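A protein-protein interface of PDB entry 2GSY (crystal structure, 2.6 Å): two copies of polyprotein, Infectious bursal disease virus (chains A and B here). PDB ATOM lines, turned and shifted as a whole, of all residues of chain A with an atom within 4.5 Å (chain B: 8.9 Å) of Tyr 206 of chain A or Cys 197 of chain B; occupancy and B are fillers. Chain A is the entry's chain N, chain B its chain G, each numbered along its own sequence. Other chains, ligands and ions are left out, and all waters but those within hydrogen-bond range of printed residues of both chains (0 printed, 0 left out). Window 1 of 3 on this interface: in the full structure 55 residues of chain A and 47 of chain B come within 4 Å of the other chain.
The side-chain hydroxyl (OH) of Tyr 98 of chain B lies within hydrogen-bond range of the guanidinium group (NH2) of Arg 204 of chain A.
The backbone NH (N) of Asn 233 of chain A lies within hydrogen-bond range of the backbone carbonyl oxygen (O) of Pro 185 of chain B.
N of Thr 196 of chain B is in hydrogen-bond range of O of Thr 207 of chain A (2.9 Å).
The backbone carbonyl oxygen (O) of Val 205 of chain A lies within hydrogen-bond range of the backbone NH (N) of Asp 198 of chain B (2.7 Å).
The side-chain hydroxyl (OG1) of Thr 207 of chain A lies within hydrogen-bond range of the side-chain carboxylate (OD2) of Asp 198 of chain B (2.7 Å).
NE of Arg 179 of chain B lies close to SG of Cys 197 of chain B (3.3 Å).
O of Asp 182 of chain B sits at hydrogen-bond distance from N of Cys 197 of chain B.
The backbone carbonyl oxygen (O) of Ala 195 of chain B sits at hydrogen-bond distance from the backbone NH (N) of Ile 184 of chain B (2.7 Å).
OD2 of Asp 198 of chain B lies within hydrogen-bond range of OG of Ser 239 of chain B, at 2.9 Å.
The side-chain hydroxyl of Ser 200 of chain B sits at hydrogen-bond distance from the side-chain carboxylate of Asp 201 of chain B (3.4 Å).
N of Val 335 of chain A lies within hydrogen-bond range of O of Tyr 206 of chain A, 2.8 Å away.
Among the printed residues, pairs that only touch across the chains: Tyr 206 of chain A with Thr 196 of chain B (3.3 Å), Thr 207 of chain A with Ala 195 of chain B (3.3 Å), Asn 233 of chain A with Ile 184 of chain B (3.4 Å), Ile 208 of chain A with Val 194 of chain B (3.4 Å), Tyr 206 of chain A with Cys 197 of chain B (3.5 Å), Val 205 of chain A with Cys 197 of chain B (3.5 Å), Arg 204 of chain A with Ser 200 of chain B (3.5 Å), Val 205 of chain A with Ser 200 of chain B (3.6 Å), Thr 207 of chain A with Val 194 of chain B (3.6 Å), Ala 334 of chain A with Val 295 of chain B (3.7 Å), Arg 204 of chain A with Cys 197 of chain B (3.7 Å), Arg 204 of chain A with Arg 179 of chain B (3.7 Å), Thr 207 of chain A with Pro 297 of chain B (3.8 Å), Tyr 206 of chain A with Ile 184 of chain B (3.9 Å) and Thr 207 of chain A with Val 295 of chain B (3.996 Å).
Tyr 206 of chain A touches three residues of chain B.
Printed residues of chain A within 4 Å of Arg 179 of chain B: Arg 204 (3.7 Å).
Of the printed residues of chain A, Pro 185 of chain B touches Asn 233 (2.9 Å).
Of chain A, only Arg 204 (3.7 Å), Val 205 (3.5 Å) and Tyr 206 (3.5 Å) come within 4 Å of Cys 197 of chain B.
Of the printed residues of chain A, Pro 297 of chain B touches Thr 207.
The nearest residue of chain B that does not touch Tyr 206 of chain A is Asp 198 of chain B (4.8 Å).
The nearest printed residue of chain A that does not touch Thr 196 of chain B is Val 205 of chain A (4.2 Å).
Of the 12 printed residues of chain A, 7 touch a printed residue of chain B.
Printed residues of chain A that touch a printed residue of chain B: Arg 204, Val 205, Tyr 206, Thr 207, Ile 208, Asn 233 and Ala 334.
Hydrophobic or aromatic side chains of chain A that line the printed part of chain B: Val 205, Tyr 206 and Ala 334.
Of the 25 printed residues of chain B, 12 touch a printed residue of chain A.
Hydrophobic or aromatic side chains of chain B that line the printed part of chain A: Tyr 98, Ile 184, Pro 185, Val 295 and Pro 297.
Among the printed residues, no Asp or Glu carboxylate lies within 4 Å of a Lys or Arg side-chain nitrogen of the other chain.
No position is printed for both chains.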
ATOM      1  N   ARG A 204      -6.274 -16.310   8.736  1.00  0.00           N
ATOM      2  CA  ARG A 204      -4.839 -16.484   8.832  1.00  0.00           C
ATOM      3  C   ARG A 204      -4.349 -15.472   9.848  1.00  0.00           C
ATOM      4  O   ARG A 204      -4.785 -14.323   9.846  1.00  0.00           O
ATOM      5  CB  ARG A 204      -4.180 -16.251   7.480  1.00  0.00           C
ATOM      6  CG  ARG A 204      -2.668 -16.296   7.532  1.00  0.00           C
ATOM      7  CD  ARG A 204      -2.055 -16.011   6.188  1.00  0.00           C
ATOM      8  NE  ARG A 204      -2.179 -17.153   5.293  1.00  0.00           N
ATOM      9  CZ  ARG A 204      -1.540 -17.268   4.134  1.00  0.00           C
ATOM     10  NH1 ARG A 204      -0.718 -16.312   3.720  1.00  0.00           N
ATOM     11  NH2 ARG A 204      -1.721 -18.349   3.389  1.00  0.00           N
ATOM     12  N   VAL A 205      -3.456 -15.907  10.726  1.00  0.00           N
ATOM     13  CA  VAL A 205      -2.905 -15.034  11.756  1.00  0.00           C
ATOM     14  C   VAL A 205      -1.383 -15.009  11.694  1.00  0.00           C
ATOM     15  O   VAL A 205      -0.733 -16.058  11.720  1.00  0.00           O
ATOM     16  CB  VAL A 205      -3.360 -15.468  13.167  1.00  0.00           C
ATOM     17  CG1 VAL A 205      -2.623 -14.685  14.237  1.00  0.00           C
ATOM     18  CG2 VAL A 205      -4.857 -15.280  13.319  1.00  0.00           C
ATOM     19  N   TYR A 206      -0.826 -13.806  11.594  1.00  0.00           N
ATOM     20  CA  TYR A 206       0.606 -13.604  11.733  1.00  0.00           C
ATOM     21  C   TYR A 206       0.882 -12.992  13.093  1.00  0.00           C
ATOM     22  O   TYR A 206       0.161 -12.100  13.535  1.00  0.00           O
ATOM     23  CB  TYR A 206       1.128 -12.645  10.676  1.00  0.00           C
ATOM     24  CG  TYR A 206       0.972 -13.092   9.248  1.00  0.00           C
ATOM     25  CD1 TYR A 206      -0.081 -12.625   8.470  1.00  0.00           C
ATOM     26  CD2 TYR A 206       1.898 -13.952   8.657  1.00  0.00           C
ATOM     27  CE1 TYR A 206      -0.219 -13.012   7.146  1.00  0.00           C
ATOM     28  CE2 TYR A 206       1.772 -14.345   7.326  1.00  0.00           C
ATOM     29  CZ  TYR A 206       0.710 -13.869   6.579  1.00  0.00           C
ATOM     30  OH  TYR A 206       0.573 -14.249   5.263  1.00  0.00           O
ATOM     31  N   THR A 207       1.926 -13.470  13.752  1.00  0.00           N
ATOM     32  CA  THR A 207       2.333 -12.908  15.026  1.00  0.00           C
ATOM     33  C   THR A 207       3.740 -12.372  14.884  1.00  0.00           C
ATOM     34  O   THR A 207       4.651 -13.090  14.477  1.00  0.00           O
ATOM     35  CB  THR A 207       2.247 -13.946  16.155  1.00  0.00           C
ATOM     36  OG1 THR A 207       0.880 -14.334  16.322  1.00  0.00           O
ATOM     37  CG2 THR A 207       2.760 -13.373  17.466  1.00  0.00           C
ATOM     38  N   ILE A 208       3.901 -11.096  15.200  1.00  0.00           N
ATOM     39  CA  ILE A 208       5.177 -10.429  15.054  1.00  0.00           C
ATOM     40  C   ILE A 208       5.576  -9.874  16.402  1.00  0.00           C
ATOM     41  O   ILE A 208       4.925  -8.977  16.928  1.00  0.00           O
ATOM     42  CB  ILE A 208       5.082  -9.288  14.028  1.00  0.00           C
ATOM     43  CG1 ILE A 208       4.638  -9.838  12.670  1.00  0.00           C
ATOM     44  CG2 ILE A 208       6.416  -8.561  13.906  1.00  0.00           C
ATOM     45  CD1 ILE A 208       4.042  -8.812  11.750  1.00  0.00           C
ATOM     46  N   ASN A 233       6.859  -9.910   5.681  1.00  0.00           N
ATOM     47  CA  ASN A 233       6.049 -10.330   4.552  1.00  0.00           C
ATOM     48  C   ASN A 233       4.765 -10.980   5.015  1.00  0.00           C
ATOM     49  O   ASN A 233       4.786 -11.940   5.785  1.00  0.00           O
ATOM     50  CB  ASN A 233       6.819 -11.312   3.674  1.00  0.00           C
ATOM     51  CG  ASN A 233       7.963 -10.660   2.927  1.00  0.00           C
ATOM     52  OD1 ASN A 233       8.071  -9.433   2.855  1.00  0.00           O
ATOM     53  ND2 ASN A 233       8.829 -11.484   2.358  1.00  0.00           N
ATOM     54  N   ILE A 234       3.641 -10.450   4.550  1.00  0.00           N
ATOM     55  CA  ILE A 234       2.342 -11.028   4.845  1.00  0.00           C
ATOM     56  C   ILE A 234       1.522 -10.990   3.572  1.00  0.00           C
ATOM     57  O   ILE A 234       1.918 -10.355   2.601  1.00  0.00           O
ATOM     58  CB  ILE A 234       1.604 -10.254   5.965  1.00  0.00           C
ATOM     59  CG1 ILE A 234       1.372  -8.793   5.563  1.00  0.00           C
ATOM     60  CG2 ILE A 234       2.366 -10.349   7.285  1.00  0.00           C
ATOM     61  CD1 ILE A 234       0.239  -8.134   6.309  1.00  0.00           C
ATOM     62  N   ASP A 235       0.373 -11.652   3.566  1.00  0.00           N
ATOM     63  CA  ASP A 235      -0.490 -11.576   2.398  1.00  0.00           C
ATOM     64  C   ASP A 235      -1.901 -11.145   2.730  1.00  0.00           C
ATOM     65  O   ASP A 235      -2.488 -11.595   3.712  1.00  0.00           O
ATOM     66  CB  ASP A 235      -0.485 -12.896   1.635  1.00  0.00           C
ATOM     67  CG  ASP A 235       0.806 -13.109   0.873  1.00  0.00           C
ATOM     68  OD1 ASP A 235       1.003 -12.444  -0.172  1.00  0.00           O
ATOM     69  OD2 ASP A 235       1.631 -13.933   1.324  1.00  0.00           O
ATOM     70  N   LEU A 333       2.572  -8.037  17.998  1.00  0.00           N
ATOM     71  CA  LEU A 333       1.374  -7.688  17.267  1.00  0.00           C
ATOM     72  C   LEU A 333       0.812  -8.924  16.597  1.00  0.00           C
ATOM     73  O   LEU A 333       1.539  -9.876  16.320  1.00  0.00           O
ATOM     74  CB  LEU A 333       1.697  -6.653  16.193  1.00  0.00           C
ATOM     75  CG  LEU A 333       2.516  -5.429  16.590  1.00  0.00           C
ATOM     76  CD1 LEU A 333       2.702  -4.543  15.377  1.00  0.00           C
ATOM     77  CD2 LEU A 333       1.836  -4.665  17.710  1.00  0.00           C
ATOM     78  N   ALA A 334      -0.486  -8.902  16.332  1.00  0.00           N
ATOM     79  CA  ALA A 334      -1.117  -9.975  15.588  1.00  0.00           C
ATOM     80  C   ALA A 334      -1.841  -9.395  14.390  1.00  0.00           C
ATOM     81  O   ALA A 334      -2.656  -8.476  14.525  1.00  0.00           O
ATOM     82  CB  ALA A 334      -2.074 -10.754  16.471  1.00  0.00           C
ATOM     83  N   VAL A 335      -1.522  -9.923  13.214  1.00  0.00           N
ATOM     84  CA  VAL A 335      -2.179  -9.504  11.989  1.00  0.00           C
ATOM     85  C   VAL A 335      -3.111 -10.624  11.577  1.00  0.00           C
ATOM     86  O   VAL A 335      -2.665 -11.720  11.245  1.00  0.00           O
ATOM     87  CB  VAL A 335      -1.161  -9.213  10.868  1.00  0.00           C
ATOM     88  CG1 VAL A 335      -1.865  -8.662   9.637  1.00  0.00           C
ATOM     89  CG2 VAL A 335      -0.091  -8.238  11.353  1.00  0.00           C
ATOM     90  N   ILE A 337      -5.697 -11.842   8.915  1.00  0.00           N
ATOM     91  CA  ILE A 337      -6.369 -11.582   7.656  1.00  0.00           C
ATOM     92  C   ILE A 337      -7.549 -12.536   7.525  1.00  0.00           C
ATOM     93  O   ILE A 337      -7.408 -13.764   7.577  1.00  0.00           O
ATOM     94  CB  ILE A 337      -5.424 -11.445   6.424  1.00  0.00           C
ATOM     95  CG1 ILE A 337      -5.033 -12.778   5.866  1.00  0.00           C
ATOM     96  CG2 ILE A 337      -4.089 -10.756   6.821  1.00  0.00           C
ATOM     97  CD1 ILE A 337      -3.710 -13.161   6.426  1.00  0.00           C
ATOM     98  N   PRO B  93       7.845 -26.768  11.740  1.00  0.00           N
ATOM     99  CA  PRO B  93       7.638 -25.427  11.177  1.00  0.00           C
ATOM    100  C   PRO B  93       8.877 -24.794  10.535  1.00  0.00           C
ATOM    101  O   PRO B  93       8.742 -23.803   9.825  1.00  0.00           O
ATOM    102  CB  PRO B  93       7.183 -24.598  12.390  1.00  0.00           C
ATOM    103  CG  PRO B  93       6.661 -25.600  13.362  1.00  0.00           C
ATOM    104  CD  PRO B  93       7.553 -26.786  13.187  1.00  0.00           C
ATOM    105  N   TYR B  96       8.210 -26.933   6.931  1.00  0.00           N
ATOM    106  CA  TYR B  96       6.885 -27.055   6.346  1.00  0.00           C
ATOM    107  C   TYR B  96       5.977 -25.927   6.826  1.00  0.00           C
ATOM    108  O   TYR B  96       6.176 -25.386   7.911  1.00  0.00           O
ATOM    109  CB  TYR B  96       6.287 -28.423   6.685  1.00  0.00           C
ATOM    110  CG  TYR B  96       7.154 -29.574   6.241  1.00  0.00           C
ATOM    111  CD1 TYR B  96       8.082 -30.146   7.111  1.00  0.00           C
ATOM    112  CD2 TYR B  96       7.063 -30.080   4.946  1.00  0.00           C
ATOM    113  CE1 TYR B  96       8.890 -31.195   6.707  1.00  0.00           C
ATOM    114  CE2 TYR B  96       7.865 -31.132   4.530  1.00  0.00           C
ATOM    115  CZ  TYR B  96       8.776 -31.685   5.413  1.00  0.00           C
ATOM    116  OH  TYR B  96       9.574 -32.730   5.009  1.00  0.00           O
ATOM    117  N   ASN B  97       4.989 -25.575   6.015  1.00  0.00           N
ATOM    118  CA  ASN B  97       4.054 -24.518   6.374  1.00  0.00           C
ATOM    119  C   ASN B  97       2.695 -25.036   6.787  1.00  0.00           C
ATOM    120  O   ASN B  97       2.002 -24.407   7.581  1.00  0.00           O
ATOM    121  CB  ASN B  97       3.888 -23.530   5.222  1.00  0.00           C
ATOM    122  CG  ASN B  97       5.061 -22.583   5.098  1.00  0.00           C
ATOM    123  OD1 ASN B  97       5.975 -22.588   5.923  1.00  0.00           O
ATOM    124  ND2 ASN B  97       5.039 -21.759   4.062  1.00  0.00           N
ATOM    125  N   TYR B  98       2.306 -26.180   6.243  1.00  0.00           N
ATOM    126  CA  TYR B  98       1.003 -26.736   6.536  1.00  0.00           C
ATOM    127  C   TYR B  98       1.132 -28.190   6.881  1.00  0.00           C
ATOM    128  O   TYR B  98       2.057 -28.866   6.427  1.00  0.00           O
ATOM    129  CB  TYR B  98       0.067 -26.567   5.345  1.00  0.00           C
ATOM    130  CG  TYR B  98      -0.338 -25.142   5.103  1.00  0.00           C
ATOM    131  CD1 TYR B  98       0.358 -24.343   4.197  1.00  0.00           C
ATOM    132  CD2 TYR B  98      -1.416 -24.581   5.789  1.00  0.00           C
ATOM    133  CE1 TYR B  98      -0.014 -23.026   3.973  1.00  0.00           C
ATOM    134  CE2 TYR B  98      -1.795 -23.267   5.571  1.00  0.00           C
ATOM    135  CZ  TYR B  98      -1.090 -22.495   4.664  1.00  0.00           C
ATOM    136  OH  TYR B  98      -1.473 -21.191   4.447  1.00  0.00           O
ATOM    137  N   VAL B 178      -3.313 -27.480   8.840  1.00  0.00           N
ATOM    138  CA  VAL B 178      -3.060 -26.507   9.882  1.00  0.00           C
ATOM    139  C   VAL B 178      -1.798 -25.771   9.521  1.00  0.00           C
ATOM    140  O   VAL B 178      -0.806 -26.400   9.155  1.00  0.00           O
ATOM    141  CB  VAL B 178      -2.851 -27.203  11.232  1.00  0.00           C
ATOM    142  CG1 VAL B 178      -2.286 -26.246  12.258  1.00  0.00           C
ATOM    143  CG2 VAL B 178      -4.143 -27.758  11.722  1.00  0.00           C
ATOM    144  N   ARG B 179      -1.807 -24.446   9.619  1.00  0.00           N
ATOM    145  CA  ARG B 179      -0.538 -23.768   9.482  1.00  0.00           C
ATOM    146  C   ARG B 179       0.332 -24.025  10.701  1.00  0.00           C
ATOM    147  O   ARG B 179      -0.109 -23.877  11.836  1.00  0.00           O
ATOM    148  CB  ARG B 179      -0.642 -22.282   9.189  1.00  0.00           C
ATOM    149  CG  ARG B 179       0.731 -21.841   8.746  1.00  0.00           C
ATOM    150  CD  ARG B 179       0.805 -20.491   8.192  1.00  0.00           C
ATOM    151  NE  ARG B 179       0.692 -20.422   6.740  1.00  0.00           N
ATOM    152  CZ  ARG B 179       1.652 -19.998   5.920  1.00  0.00           C
ATOM    153  NH1 ARG B 179       2.847 -19.636   6.376  1.00  0.00           N
ATOM    154  NH2 ARG B 179       1.403 -19.942   4.622  1.00  0.00           N
ATOM    155  N   LEU B 180       1.567 -24.437  10.456  1.00  0.00           N
ATOM    156  CA  LEU B 180       2.499 -24.679  11.544  1.00  0.00           C
ATOM    157  C   LEU B 180       2.958 -23.313  12.029  1.00  0.00           C
ATOM    158  O   LEU B 180       2.610 -22.303  11.425  1.00  0.00           O
ATOM    159  CB  LEU B 180       3.649 -25.543  11.041  1.00  0.00           C
ATOM    160  CG  LEU B 180       3.150 -26.911  10.551  1.00  0.00           C
ATOM    161  CD1 LEU B 180       4.003 -27.449   9.417  1.00  0.00           C
ATOM    162  CD2 LEU B 180       3.064 -27.909  11.702  1.00  0.00           C
ATOM    163  N   GLY B 181       3.710 -23.221  13.108  1.00  0.00           N
ATOM    164  CA  GLY B 181       4.103 -21.873  13.518  1.00  0.00           C
ATOM    165  C   GLY B 181       5.309 -21.381  12.747  1.00  0.00           C
ATOM    166  O   GLY B 181       6.295 -20.964  13.355  1.00  0.00           O
ATOM    167  N   ASP B 182       5.240 -21.421  11.417  1.00  0.00           N
ATOM    168  CA  ASP B 182       6.439 -21.250  10.589  1.00  0.00           C
ATOM    169  C   ASP B 182       6.960 -19.812  10.539  1.00  0.00           C
ATOM    170  O   ASP B 182       6.175 -18.872  10.486  1.00  0.00           O
ATOM    171  CB  ASP B 182       6.203 -21.783   9.174  1.00  0.00           C
ATOM    172  CG  ASP B 182       5.167 -20.991   8.417  1.00  0.00           C
ATOM    173  OD1 ASP B 182       3.961 -21.199   8.669  1.00  0.00           O
ATOM    174  OD2 ASP B 182       5.567 -20.162   7.568  1.00  0.00           O
ATOM    175  N   PRO B 183       8.294 -19.641  10.558  1.00  0.00           N
ATOM    176  CA  PRO B 183       8.864 -18.298  10.480  1.00  0.00           C
ATOM    177  C   PRO B 183       8.543 -17.660   9.141  1.00  0.00           C
ATOM    178  O   PRO B 183       8.530 -18.342   8.117  1.00  0.00           O
ATOM    179  CB  PRO B 183      10.372 -18.538  10.615  1.00  0.00           C
ATOM    180  CG  PRO B 183      10.574 -19.941  10.218  1.00  0.00           C
ATOM    181  CD  PRO B 183       9.345 -20.668  10.663  1.00  0.00           C
ATOM    182  N   ILE B 184       8.265 -16.363   9.167  1.00  0.00           N
ATOM    183  CA  ILE B 184       7.878 -15.629   7.975  1.00  0.00           C
ATOM    184  C   ILE B 184       9.021 -14.653   7.657  1.00  0.00           C
ATOM    185  O   ILE B 184       9.697 -14.190   8.577  1.00  0.00           O
ATOM    186  CB  ILE B 184       6.461 -14.977   8.182  1.00  0.00           C
ATOM    187  CG1 ILE B 184       5.624 -15.061   6.909  1.00  0.00           C
ATOM    188  CG2 ILE B 184       6.523 -13.556   8.740  1.00  0.00           C
ATOM    189  CD1 ILE B 184       5.248 -16.491   6.520  1.00  0.00           C
ATOM    190  N   PRO B 185       9.293 -14.386   6.363  1.00  0.00           N
ATOM    191  CA  PRO B 185      10.430 -13.493   6.103  1.00  0.00           C
ATOM    192  C   PRO B 185      10.198 -12.120   6.721  1.00  0.00           C
ATOM    193  O   PRO B 185       9.139 -11.518   6.521  1.00  0.00           O
ATOM    194  CB  PRO B 185      10.473 -13.383   4.575  1.00  0.00           C
ATOM    195  CG  PRO B 185       9.676 -14.513   4.067  1.00  0.00           C
ATOM    196  CD  PRO B 185       8.649 -14.841   5.118  1.00  0.00           C
ATOM    197  N   VAL B 194      10.773 -11.900  16.139  1.00  0.00           N
ATOM    198  CA  VAL B 194      10.251 -13.177  15.681  1.00  0.00           C
ATOM    199  C   VAL B 194       8.931 -12.953  14.953  1.00  0.00           C
ATOM    200  O   VAL B 194       8.028 -12.301  15.478  1.00  0.00           O
ATOM    201  CB  VAL B 194      10.064 -14.146  16.867  1.00  0.00           C
ATOM    202  CG1 VAL B 194       9.250 -15.373  16.461  1.00  0.00           C
ATOM    203  CG2 VAL B 194      11.420 -14.558  17.432  1.00  0.00           C
ATOM    204  N   ALA B 195       8.826 -13.481  13.739  1.00  0.00           N
ATOM    205  CA  ALA B 195       7.610 -13.330  12.953  1.00  0.00           C
ATOM    206  C   ALA B 195       7.161 -14.673  12.401  1.00  0.00           C
ATOM    207  O   ALA B 195       7.878 -15.315  11.637  1.00  0.00           O
ATOM    208  CB  ALA B 195       7.823 -12.333  11.834  1.00  0.00           C
ATOM    209  N   THR B 196       5.969 -15.101  12.794  1.00  0.00           N
ATOM    210  CA  THR B 196       5.467 -16.397  12.366  1.00  0.00           C
ATOM    211  C   THR B 196       4.067 -16.284  11.793  1.00  0.00           C
ATOM    212  O   THR B 196       3.408 -15.258  11.939  1.00  0.00           O
ATOM    213  CB  THR B 196       5.448 -17.424  13.524  1.00  0.00           C
ATOM    214  OG1 THR B 196       4.624 -16.929  14.584  1.00  0.00           O
ATOM    215  CG2 THR B 196       6.846 -17.683  14.056  1.00  0.00           C
ATOM    216  N   CYS B 197       3.632 -17.348  11.130  1.00  0.00           N
ATOM    217  CA  CYS B 197       2.276 -17.458  10.637  1.00  0.00           C
ATOM    218  C   CYS B 197       1.660 -18.626  11.389  1.00  0.00           C
ATOM    219  O   CYS B 197       2.098 -19.759  11.228  1.00  0.00           O
ATOM    220  CB  CYS B 197       2.295 -17.720   9.136  1.00  0.00           C
ATOM    221  SG  CYS B 197       0.705 -17.482   8.324  1.00  0.00           S
ATOM    222  N   ASP B 198       0.663 -18.356  12.220  1.00  0.00           N
ATOM    223  CA  ASP B 198       0.264 -19.324  13.239  1.00  0.00           C
ATOM    224  C   ASP B 198      -0.943 -20.171  12.892  1.00  0.00           C
ATOM    225  O   ASP B 198      -1.760 -19.793  12.047  1.00  0.00           O
ATOM    226  CB  ASP B 198       0.004 -18.606  14.557  1.00  0.00           C
ATOM    227  CG  ASP B 198       1.230 -17.904  15.090  1.00  0.00           C
ATOM    228  OD1 ASP B 198       2.365 -18.245  14.675  1.00  0.00           O
ATOM    229  OD2 ASP B 198       1.052 -17.005  15.938  1.00  0.00           O
ATOM    230  N   SER B 199      -1.052 -21.318  13.559  1.00  0.00           N
ATOM    231  CA  SER B 199      -2.280 -22.098  13.539  1.00  0.00           C
ATOM    232  C   SER B 199      -3.393 -21.182  13.968  1.00  0.00           C
ATOM    233  O   SER B 199      -3.374 -20.655  15.079  1.00  0.00           O
ATOM    234  CB  SER B 199      -2.202 -23.257  14.516  1.00  0.00           C
ATOM    235  OG  SER B 199      -0.991 -23.954  14.343  1.00  0.00           O
ATOM    236  N   SER B 200      -4.358 -20.989  13.085  1.00  0.00           N
ATOM    237  CA  SER B 200      -5.384 -20.002  13.319  1.00  0.00           C
ATOM    238  C   SER B 200      -6.777 -20.549  13.093  1.00  0.00           C
ATOM    239  O   SER B 200      -7.676 -20.284  13.892  1.00  0.00           O
ATOM    240  CB  SER B 200      -5.136 -18.780  12.440  1.00  0.00           C
ATOM    241  OG  SER B 200      -4.844 -19.165  11.108  1.00  0.00           O
ATOM    242  N   ASP B 201      -6.959 -21.312  12.011  1.00  0.00           N
ATOM    243  CA  ASP B 201      -8.272 -21.857  11.663  1.00  0.00           C
ATOM    244  C   ASP B 201      -8.862 -22.519  12.887  1.00  0.00           C
ATOM    245  O   ASP B 201      -8.165 -23.236  13.607  1.00  0.00           O
ATOM    246  CB  ASP B 201      -8.192 -22.899  10.539  1.00  0.00           C
ATOM    247  CG  ASP B 201      -7.181 -22.544   9.454  1.00  0.00           C
ATOM    248  OD1 ASP B 201      -6.107 -21.984   9.769  1.00  0.00           O
ATOM    249  OD2 ASP B 201      -7.452 -22.858   8.276  1.00  0.00           O
ATOM    250  N   SER B 239       0.285 -19.674  20.357  1.00  0.00           N
ATOM    251  CA  SER B 239      -0.091 -18.263  20.476  1.00  0.00           C
ATOM    252  C   SER B 239      -1.557 -18.014  20.827  1.00  0.00           C
ATOM    253  O   SER B 239      -2.450 -18.739  20.387  1.00  0.00           O
ATOM    254  CB  SER B 239       0.264 -17.501  19.201  1.00  0.00           C
ATOM    255  OG  SER B 239      -0.604 -17.858  18.144  1.00  0.00           O
ATOM    256  N   VAL B 295      -1.143  -9.804  22.922  1.00  0.00           N
ATOM    257  CA  VAL B 295      -0.821 -10.880  22.001  1.00  0.00           C
ATOM    258  C   VAL B 295       0.332 -11.667  22.608  1.00  0.00           C
ATOM    259  O   VAL B 295       1.388 -11.104  22.918  1.00  0.00           O
ATOM    260  CB  VAL B 295      -0.455 -10.347  20.603  1.00  0.00           C
ATOM    261  CG1 VAL B 295       0.071 -11.467  19.725  1.00  0.00           C
ATOM    262  CG2 VAL B 295      -1.659  -9.703  19.954  1.00  0.00           C
ATOM    263  N   PRO B 297       2.935 -14.562  21.872  1.00  0.00           N
ATOM    264  CA  PRO B 297       3.523 -15.406  20.838  1.00  0.00           C
ATOM    265  C   PRO B 297       3.851 -16.802  21.357  1.00  0.00           C
ATOM    266  O   PRO B 297       4.133 -16.970  22.544  1.00  0.00           O
ATOM    267  CB  PRO B 297       4.804 -14.660  20.464  1.00  0.00           C
ATOM    268  CG  PRO B 297       5.156 -13.884  21.679  1.00  0.00           C
ATOM    269  CD  PRO B 297       3.869 -13.525  22.347  1.00  0.00           C
ATOM    270  N   THR B 298       3.813 -17.784  20.462  1.00  0.00           N
ATOM    271  CA  THR B 298       4.145 -19.168  20.793  1.00  0.00           C
ATOM    272  C   THR B 298       5.449 -19.323  21.583  1.00  0.00           C
ATOM    273  O   THR B 298       5.484 -20.030  22.586  1.00  0.00           O
ATOM    274  CB  THR B 298       4.193 -20.036  19.518  1.00  0.00           C
ATOM    275  OG1 THR B 298       2.901 -20.032  18.896  1.00  0.00           O
ATOM    276  CG2 THR B 298       4.582 -21.471  19.846  1.00  0.00           C
ATOM    277  N   HIS B 338      -5.428 -19.257  19.260  1.00  0.00           N
ATOM    278  CA  HIS B 338      -5.440 -19.439  17.825  1.00  0.00           C
ATOM    279  C   HIS B 338      -5.361 -20.909  17.456  1.00  0.00           C
ATOM    280  O   HIS B 338      -4.538 -21.657  17.988  1.00  0.00           O
ATOM    281  CB  HIS B 338      -4.319 -18.617  17.198  1.00  0.00           C
ATOM    282  CG  HIS B 338      -4.407 -17.157  17.514  1.00  0.00           C
ATOM    283  ND1 HIS B 338      -5.475 -16.376  17.120  1.00  0.00           N
ATOM    284  CD2 HIS B 338      -3.572 -16.336  18.195  1.00  0.00           C
ATOM    285  CE1 HIS B 338      -5.290 -15.138  17.539  1.00  0.00           C
ATOM    286  NE2 HIS B 338      -4.143 -15.086  18.194  1.00  0.00           N
